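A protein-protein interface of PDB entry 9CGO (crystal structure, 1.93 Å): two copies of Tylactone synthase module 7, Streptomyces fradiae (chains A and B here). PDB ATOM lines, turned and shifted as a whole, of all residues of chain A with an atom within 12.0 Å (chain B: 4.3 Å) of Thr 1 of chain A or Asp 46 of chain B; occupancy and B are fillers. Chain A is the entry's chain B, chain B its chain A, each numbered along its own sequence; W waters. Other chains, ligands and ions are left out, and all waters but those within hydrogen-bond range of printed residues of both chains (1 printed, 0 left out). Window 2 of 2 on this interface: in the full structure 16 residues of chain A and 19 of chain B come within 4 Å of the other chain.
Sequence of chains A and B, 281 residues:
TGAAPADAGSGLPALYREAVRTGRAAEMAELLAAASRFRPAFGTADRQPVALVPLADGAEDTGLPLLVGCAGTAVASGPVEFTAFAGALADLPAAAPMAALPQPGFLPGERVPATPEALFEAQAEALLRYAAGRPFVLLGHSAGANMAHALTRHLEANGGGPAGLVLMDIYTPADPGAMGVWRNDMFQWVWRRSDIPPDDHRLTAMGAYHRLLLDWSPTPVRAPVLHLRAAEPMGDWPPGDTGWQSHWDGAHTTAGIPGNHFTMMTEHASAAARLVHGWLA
Printed residues of chain A within 4 Å of Asp 46 of chain B: Thr 1 (3.7 Å). Of the printed residues of chain A, Pro 40 of chain B touches Thr 1 (3.8 Å) and Gly 2 (3.9 Å). Of chain A, only Thr 1 comes within 4 Å of Ala 41 of chain B. No residue of chain A comes within 4 Å of Thr 44 of chain B. Ala 45 of chain B touches none of the printed residues of chain A. Of the printed residues of chain A, Arg 111 of chain B touches Thr 1. Of the printed residues of chain B, Gly 2 of chain A touches Pro 40. Arg 24 of chain A touches none of the printed residues of chain B. Arg 21 of chain A touches none of the printed residues of chain B. The nearest printed residue of chain B that does not touch Thr 1 of chain A is Phe 42 of chain B (5.1 Å). The nearest printed residue of chain B that does not touch Gly 2 of chain A is Ala 41 of chain B (4.7 Å).
Among the printed residues, pairs that only touch across the chains: Thr 1 of chain A with Pro 40 of chain B (3.8 Å), Thr 1 of chain A with Asp 46 of chain B (3.7 Å) and Gly 2 of chain A with Pro 40 of chain B (3.9 Å).
Water W1 lies within hydrogen-bond range of OD2 of Asp 46 of chain B (2.7 Å), OG1 of Thr 1 of chain A (3.0 Å) and N of Gly 43 of chain B (3.5 Å).
O of Ala 41 of chain B lies within hydrogen-bond range of NH2 of Arg 111 of chain B, at 2.5 Å. The backbone NH (N) of Gly 43 of chain B sits at hydrogen-bond distance from the side-chain carboxylate (OD1) of Asp 46 of chain B, at 2.6 Å. The side-chain carboxylate of Asp 46 of chain B lies within salt-bridge range of the guanidinium group of Arg 111 of chain B. N of Arg 111 of chain B is in hydrogen-bond range of OE1 of Gln 48 of chain B (2.7 Å).
Along chain A the printed residues that touch a printed residue of chain B span positions 1 to 2. Along chain B the printed residues that touch a printed residue of chain A span positions 40 to 111. Among the printed residues, 5 pairs touch across the chains. Among the printed residues, no Asp or Glu carboxylate lies within 4 Å of a Lys or Arg side-chain nitrogen of the other chain.
O of Thr 1 of chain A is in hydrogen-bond range of NH2 of Arg 111 of chain B (3.0 Å). The backbone NH (N) of Ala 41 of chain B sits close to the backbone NH (N) of Thr 1 of chain A.
No position is printed for both chains. Of the 5 pairs that touch across the chains among the printed residues, none has its exchanged pair printed and touching as well.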
ATOM      1  N   THR A   1      22.648 -10.753  14.017  1.00  0.00           N
ATOM      2  CA  THR A   1      22.722 -12.011  14.750  1.00  0.00           C
ATOM      3  C   THR A   1      24.089 -12.721  14.675  1.00  0.00           C
ATOM      4  O   THR A   1      24.445 -13.435  15.611  1.00  0.00           O
ATOM      5  CB  THR A   1      21.614 -12.961  14.294  1.00  0.00           C
ATOM      6  OG1 THR A   1      21.946 -14.316  14.629  1.00  0.00           O
ATOM      7  CG2 THR A   1      21.372 -12.818  12.822  1.00  0.00           C
ATOM      8  N   GLY A   2      24.846 -12.532  13.583  1.00  0.00           N
ATOM      9  CA  GLY A   2      26.272 -12.830  13.595  1.00  0.00           C
ATOM     10  C   GLY A   2      26.819 -13.610  12.407  1.00  0.00           C
ATOM     11  O   GLY A   2      26.679 -14.829  12.348  1.00  0.00           O
ATOM     12  N   ALA A   3      27.453 -12.922  11.447  1.00  0.00           N
ATOM     13  CA  ALA A   3      27.908 -13.577  10.224  1.00  0.00           C
ATOM     14  C   ALA A   3      29.289 -14.206  10.338  1.00  0.00           C
ATOM     15  O   ALA A   3      29.608 -15.111   9.559  1.00  0.00           O
ATOM     16  CB  ALA A   3      27.924 -12.586   9.058  1.00  0.00           C
ATOM     17  N   ALA A   4      30.122 -13.750  11.267  1.00  0.00           N
ATOM     18  CA  ALA A   4      31.456 -14.318  11.456  1.00  0.00           C
ATOM     19  C   ALA A   4      31.870 -14.118  12.902  1.00  0.00           C
ATOM     20  O   ALA A   4      32.536 -13.136  13.252  1.00  0.00           O
ATOM     21  CB  ALA A   4      32.471 -13.687  10.502  1.00  0.00           C
ATOM     22  N   PRO A   5      31.473 -15.038  13.783  1.00  0.00           N
ATOM     23  CA  PRO A   5      31.788 -14.878  15.214  1.00  0.00           C
ATOM     24  C   PRO A   5      33.272 -14.804  15.504  1.00  0.00           C
ATOM     25  O   PRO A   5      33.668 -14.203  16.512  1.00  0.00           O
ATOM     26  CB  PRO A   5      31.151 -16.124  15.847  1.00  0.00           C
ATOM     27  CG  PRO A   5      30.078 -16.529  14.878  1.00  0.00           C
ATOM     28  CD  PRO A   5      30.656 -16.231  13.528  1.00  0.00           C
ATOM     29  N   ALA A   6      34.105 -15.391  14.641  1.00  0.00           N
ATOM     30  CA  ALA A   6      35.554 -15.339  14.803  1.00  0.00           C
ATOM     31  C   ALA A   6      36.105 -13.921  14.859  1.00  0.00           C
ATOM     32  O   ALA A   6      37.216 -13.723  15.359  1.00  0.00           O
ATOM     33  CB  ALA A   6      36.223 -16.098  13.663  1.00  0.00           C
ATOM     34  N   ASP A   7      35.376 -12.936  14.350  1.00  0.00           N
ATOM     35  CA  ASP A   7      35.836 -11.553  14.410  1.00  0.00           C
ATOM     36  C   ASP A   7      35.640 -11.019  15.827  1.00  0.00           C
ATOM     37  O   ASP A   7      34.540 -11.113  16.384  1.00  0.00           O
ATOM     38  CB  ASP A   7      35.063 -10.705  13.391  1.00  0.00           C
ATOM     39  CG  ASP A   7      35.805  -9.433  12.972  1.00  0.00           C
ATOM     40  OD1 ASP A   7      36.307  -8.697  13.849  1.00  0.00           O
ATOM     41  OD2 ASP A   7      35.871  -9.164  11.748  1.00  0.00           O
ATOM     42  N   ALA A  14      35.067  -3.200  12.568  1.00  0.00           N
ATOM     43  CA  ALA A  14      34.279  -4.414  12.750  1.00  0.00           C
ATOM     44  C   ALA A  14      32.846  -4.218  12.266  1.00  0.00           C
ATOM     45  O   ALA A  14      32.275  -5.100  11.618  1.00  0.00           O
ATOM     46  CB  ALA A  14      34.305  -4.849  14.220  1.00  0.00           C
ATOM     47  N   LEU A  15      32.256  -3.066  12.559  1.00  0.00           N
ATOM     48  CA  LEU A  15      30.932  -2.770  12.038  1.00  0.00           C
ATOM     49  C   LEU A  15      30.952  -2.721  10.514  1.00  0.00           C
ATOM     50  O   LEU A  15      30.019  -3.191   9.852  1.00  0.00           O
ATOM     51  CB  LEU A  15      30.440  -1.448  12.632  1.00  0.00           C
ATOM     52  CG  LEU A  15      30.225  -1.524  14.150  1.00  0.00           C
ATOM     53  CD1 LEU A  15      29.839  -0.166  14.692  1.00  0.00           C
ATOM     54  CD2 LEU A  15      29.150  -2.571  14.470  1.00  0.00           C
ATOM     55  N   ARG A  17      33.056  -4.463   8.544  1.00  0.00           N
ATOM     56  CA  ARG A  17      33.124  -5.851   8.124  1.00  0.00           C
ATOM     57  C   ARG A  17      31.761  -6.519   8.198  1.00  0.00           C
ATOM     58  O   ARG A  17      31.361  -7.224   7.268  1.00  0.00           O
ATOM     59  CB  ARG A  17      34.161  -6.597   8.964  1.00  0.00           C
ATOM     60  CG  ARG A  17      35.573  -6.044   8.767  1.00  0.00           C
ATOM     61  CD  ARG A  17      36.640  -6.930   9.401  1.00  0.00           C
ATOM     62  NE  ARG A  17      36.676  -6.815  10.854  1.00  0.00           N
ATOM     63  CZ  ARG A  17      37.503  -6.020  11.520  1.00  0.00           C
ATOM     64  NH1 ARG A  17      38.402  -5.276  10.896  1.00  0.00           N
ATOM     65  NH2 ARG A  17      37.430  -5.970  12.847  1.00  0.00           N
ATOM     66  N   GLU A  18      31.006  -6.276   9.273  1.00  0.00           N
ATOM     67  CA  GLU A  18      29.706  -6.930   9.396  1.00  0.00           C
ATOM     68  C   GLU A  18      28.706  -6.418   8.362  1.00  0.00           C
ATOM     69  O   GLU A  18      27.873  -7.190   7.874  1.00  0.00           O
ATOM     70  CB  GLU A  18      29.162  -6.759  10.816  1.00  0.00           C
ATOM     71  CG  GLU A  18      28.074  -7.747  11.211  1.00  0.00           C
ATOM     72  CD  GLU A  18      28.534  -9.205  11.185  1.00  0.00           C
ATOM     73  OE1 GLU A  18      29.747  -9.461  11.006  1.00  0.00           O
ATOM     74  OE2 GLU A  18      27.675 -10.103  11.351  1.00  0.00           O
ATOM     75  N   ALA A  19      28.788  -5.137   8.002  1.00  0.00           N
ATOM     76  CA  ALA A  19      28.011  -4.616   6.876  1.00  0.00           C
ATOM     77  C   ALA A  19      28.301  -5.383   5.587  1.00  0.00           C
ATOM     78  O   ALA A  19      27.386  -5.882   4.924  1.00  0.00           O
ATOM     79  CB  ALA A  19      28.311  -3.128   6.686  1.00  0.00           C
ATOM     80  N   ARG A  21      29.681  -8.242   5.071  1.00  0.00           N
ATOM     81  CA  ARG A  21      29.326  -9.656   5.168  1.00  0.00           C
ATOM     82  C   ARG A  21      27.822  -9.881   5.005  1.00  0.00           C
ATOM     83  O   ARG A  21      27.399 -10.966   4.591  1.00  0.00           O
ATOM     84  CB  ARG A  21      29.807 -10.235   6.508  1.00  0.00           C
ATOM     85  CG  ARG A  21      31.327 -10.227   6.705  1.00  0.00           C
ATOM     86  CD  ARG A  21      31.824 -11.071   7.920  1.00  0.00           C
ATOM     87  NE  ARG A  21      31.639 -10.421   9.211  1.00  0.00           N
ATOM     88  CZ  ARG A  21      32.613  -9.979   9.998  1.00  0.00           C
ATOM     89  NH1 ARG A  21      33.891 -10.155   9.696  1.00  0.00           N
ATOM     90  NH2 ARG A  21      32.297  -9.351  11.124  1.00  0.00           N
ATOM     91  N   THR A  22      26.997  -8.885   5.326  1.00  0.00           N
ATOM     92  CA  THR A  22      25.549  -9.041   5.262  1.00  0.00           C
ATOM     93  C   THR A  22      24.914  -8.192   4.159  1.00  0.00           C
ATOM     94  O   THR A  22      23.705  -7.954   4.183  1.00  0.00           O
ATOM     95  CB  THR A  22      24.930  -8.728   6.629  1.00  0.00           C
ATOM     96  OG1 THR A  22      25.513  -7.530   7.156  1.00  0.00           O
ATOM     97  CG2 THR A  22      25.215  -9.859   7.595  1.00  0.00           C
ATOM     98  N   GLY A  23      25.701  -7.735   3.193  1.00  0.00           N
ATOM     99  CA  GLY A  23      25.140  -7.072   2.031  1.00  0.00           C
ATOM    100  C   GLY A  23      24.576  -5.690   2.279  1.00  0.00           C
ATOM    101  O   GLY A  23      23.692  -5.247   1.539  1.00  0.00           O
ATOM    102  N   ARG A  24      25.078  -4.984   3.292  1.00  0.00           N
ATOM    103  CA  ARG A  24      24.546  -3.672   3.643  1.00  0.00           C
ATOM    104  C   ARG A  24      25.607  -2.590   3.508  1.00  0.00           C
ATOM    105  O   ARG A  24      25.859  -1.837   4.456  1.00  0.00           O
ATOM    106  CB  ARG A  24      24.006  -3.692   5.077  1.00  0.00           C
ATOM    107  CG  ARG A  24      23.108  -4.855   5.356  1.00  0.00           C
ATOM    108  CD  ARG A  24      23.209  -5.310   6.814  1.00  0.00           C
ATOM    109  NE  ARG A  24      22.282  -4.622   7.700  1.00  0.00           N
ATOM    110  CZ  ARG A  24      22.243  -4.795   9.016  1.00  0.00           C
ATOM    111  NH1 ARG A  24      23.104  -5.590   9.632  1.00  0.00           N
ATOM    112  NH2 ARG A  24      21.327  -4.147   9.731  1.00  0.00           N
ATOM    113  N   GLU A  27      23.720   0.899   3.655  1.00  0.00           N
ATOM    114  CA  GLU A  27      23.391   1.323   5.015  1.00  0.00           C
ATOM    115  C   GLU A  27      24.637   1.839   5.724  1.00  0.00           C
ATOM    116  O   GLU A  27      24.613   2.915   6.324  1.00  0.00           O
ATOM    117  CB  GLU A  27      22.743   0.179   5.804  1.00  0.00           C
ATOM    118  CG  GLU A  27      22.157   0.615   7.162  1.00  0.00           C
ATOM    119  CD  GLU A  27      21.533  -0.525   7.977  1.00  0.00           C
ATOM    120  OE1 GLU A  27      21.531  -1.689   7.525  1.00  0.00           O
ATOM    121  OE2 GLU A  27      21.029  -0.242   9.082  1.00  0.00           O
ATOM    122  N   PRO B  40      25.946  -7.909  16.173  1.00  0.00           N
ATOM    123  CA  PRO B  40      25.340  -9.238  16.227  1.00  0.00           C
ATOM    124  C   PRO B  40      24.383  -9.305  17.405  1.00  0.00           C
ATOM    125  O   PRO B  40      24.667  -8.788  18.488  1.00  0.00           O
ATOM    126  CB  PRO B  40      26.539 -10.175  16.412  1.00  0.00           C
ATOM    127  CG  PRO B  40      27.691  -9.411  15.846  1.00  0.00           C
ATOM    128  CD  PRO B  40      27.415  -7.966  16.162  1.00  0.00           C
ATOM    129  N   ALA B  41      23.238  -9.931  17.175  1.00  0.00           N
ATOM    130  CA  ALA B  41      22.119  -9.915  18.105  1.00  0.00           C
ATOM    131  C   ALA B  41      21.700 -11.338  18.424  1.00  0.00           C
ATOM    132  O   ALA B  41      21.951 -12.257  17.646  1.00  0.00           O
ATOM    133  CB  ALA B  41      20.934  -9.147  17.535  1.00  0.00           C
ATOM    134  N   PHE B  42      21.072 -11.528  19.580  1.00  0.00           N
ATOM    135  CA  PHE B  42      20.516 -12.829  19.914  1.00  0.00           C
ATOM    136  C   PHE B  42      18.998 -12.763  19.883  1.00  0.00           C
ATOM    137  O   PHE B  42      18.401 -11.779  20.318  1.00  0.00           O
ATOM    138  CB  PHE B  42      21.039 -13.353  21.270  1.00  0.00           C
ATOM    139  CG  PHE B  42      20.620 -12.555  22.488  1.00  0.00           C
ATOM    140  CD1 PHE B  42      19.486 -12.914  23.209  1.00  0.00           C
ATOM    141  CD2 PHE B  42      21.398 -11.493  22.959  1.00  0.00           C
ATOM    142  CE1 PHE B  42      19.101 -12.207  24.371  1.00  0.00           C
ATOM    143  CE2 PHE B  42      21.025 -10.788  24.119  1.00  0.00           C
ATOM    144  CZ  PHE B  42      19.880 -11.148  24.829  1.00  0.00           C
ATOM    145  N   GLY B  43      18.383 -13.795  19.315  1.00  0.00           N
ATOM    146  CA  GLY B  43      16.946 -13.916  19.290  1.00  0.00           C
ATOM    147  C   GLY B  43      16.466 -14.792  20.426  1.00  0.00           C
ATOM    148  O   GLY B  43      17.222 -15.177  21.318  1.00  0.00           O
ATOM    149  N   THR B  44      15.178 -15.112  20.384  1.00  0.00           N
ATOM    150  CA  THR B  44      14.634 -16.039  21.364  1.00  0.00           C
ATOM    151  C   THR B  44      15.132 -17.454  21.115  1.00  0.00           C
ATOM    152  O   THR B  44      15.272 -18.238  22.060  1.00  0.00           O
ATOM    153  CB  THR B  44      13.102 -15.985  21.344  1.00  0.00           C
ATOM    154  OG1 THR B  44      12.563 -17.153  21.967  1.00  0.00           O
ATOM    155  CG2 THR B  44      12.597 -15.896  19.924  1.00  0.00           C
ATOM    156  N   ALA B  45      15.436 -17.789  19.859  1.00  0.00           N
ATOM    157  CA  ALA B  45      15.916 -19.132  19.551  1.00  0.00           C
ATOM    158  C   ALA B  45      17.334 -19.351  20.069  1.00  0.00           C
ATOM    159  O   ALA B  45      17.626 -20.383  20.682  1.00  0.00           O
ATOM    160  CB  ALA B  45      15.842 -19.383  18.045  1.00  0.00           C
ATOM    161  N   ASP B  46      18.227 -18.393  19.846  1.00  0.00           N
ATOM    162  CA  ASP B  46      19.639 -18.551  20.202  1.00  0.00           C
ATOM    163  C   ASP B  46      19.996 -17.684  21.410  1.00  0.00           C
ATOM    164  O   ASP B  46      20.861 -16.814  21.363  1.00  0.00           O
ATOM    165  CB  ASP B  46      20.529 -18.230  19.000  1.00  0.00           C
ATOM    166  CG  ASP B  46      20.306 -16.826  18.456  1.00  0.00           C
ATOM    167  OD1 ASP B  46      19.359 -16.155  18.921  1.00  0.00           O
ATOM    168  OD2 ASP B  46      21.079 -16.393  17.572  1.00  0.00           O
ATOM    169  N   ARG B  47      19.325 -17.957  22.523  1.00  0.00           N
ATOM    170  CA  ARG B  47      19.329 -17.016  23.633  1.00  0.00           C
ATOM    171  C   ARG B  47      20.692 -16.957  24.315  1.00  0.00           C
ATOM    172  O   ARG B  47      21.349 -17.981  24.531  1.00  0.00           O
ATOM    173  CB  ARG B  47      18.252 -17.397  24.643  1.00  0.00           C
ATOM    174  CG  ARG B  47      17.482 -16.212  25.177  1.00  0.00           C
ATOM    175  CD  ARG B  47      16.049 -16.609  25.480  1.00  0.00           C
ATOM    176  NE  ARG B  47      15.964 -17.582  26.563  1.00  0.00           N
ATOM    177  CZ  ARG B  47      14.883 -18.303  26.830  1.00  0.00           C
ATOM    178  NH1 ARG B  47      13.790 -18.212  26.084  1.00  0.00           N
ATOM    179  NH2 ARG B  47      14.899 -19.138  27.863  1.00  0.00           N
ATOM    180  N   GLN B  48      21.129 -15.738  24.632  1.00  0.00           N
ATOM    181  CA  GLN B  48      22.358 -15.534  25.387  1.00  0.00           C
ATOM    182  C   GLN B  48      22.033 -15.603  26.873  1.00  0.00           C
ATOM    183  O   GLN B  48      21.148 -14.869  27.331  1.00  0.00           O
ATOM    184  CB  GLN B  48      22.980 -14.190  25.041  1.00  0.00           C
ATOM    185  CG  GLN B  48      24.339 -13.923  25.653  1.00  0.00           C
ATOM    186  CD  GLN B  48      24.876 -12.564  25.260  1.00  0.00           C
ATOM    187  OE1 GLN B  48      25.239 -12.330  24.097  1.00  0.00           O
ATOM    188  NE2 GLN B  48      24.925 -11.649  26.226  1.00  0.00           N
ATOM    189  N   ARG B 111      26.600 -10.271  22.908  1.00  0.00           N
ATOM    190  CA  ARG B 111      25.724  -9.755  21.868  1.00  0.00           C
ATOM    191  C   ARG B 111      24.552  -8.996  22.481  1.00  0.00           C
ATOM    192  O   ARG B 111      24.230  -9.143  23.659  1.00  0.00           O
ATOM    193  CB  ARG B 111      25.202 -10.886  20.987  1.00  0.00           C
ATOM    194  CG  ARG B 111      26.295 -11.582  20.217  1.00  0.00           C
ATOM    195  CD  ARG B 111      25.929 -13.015  20.018  1.00  0.00           C
ATOM    196  NE  ARG B 111      24.835 -13.199  19.078  1.00  0.00           N
ATOM    197  CZ  ARG B 111      24.032 -14.255  19.089  1.00  0.00           C
ATOM    198  NH1 ARG B 111      24.131 -15.185  20.026  1.00  0.00           N
ATOM    199  NH2 ARG B 111      23.097 -14.372  18.148  1.00  0.00           N
HETATM  200  O   HOH W   1      19.393 -14.873  16.180  1.00  0.00           O
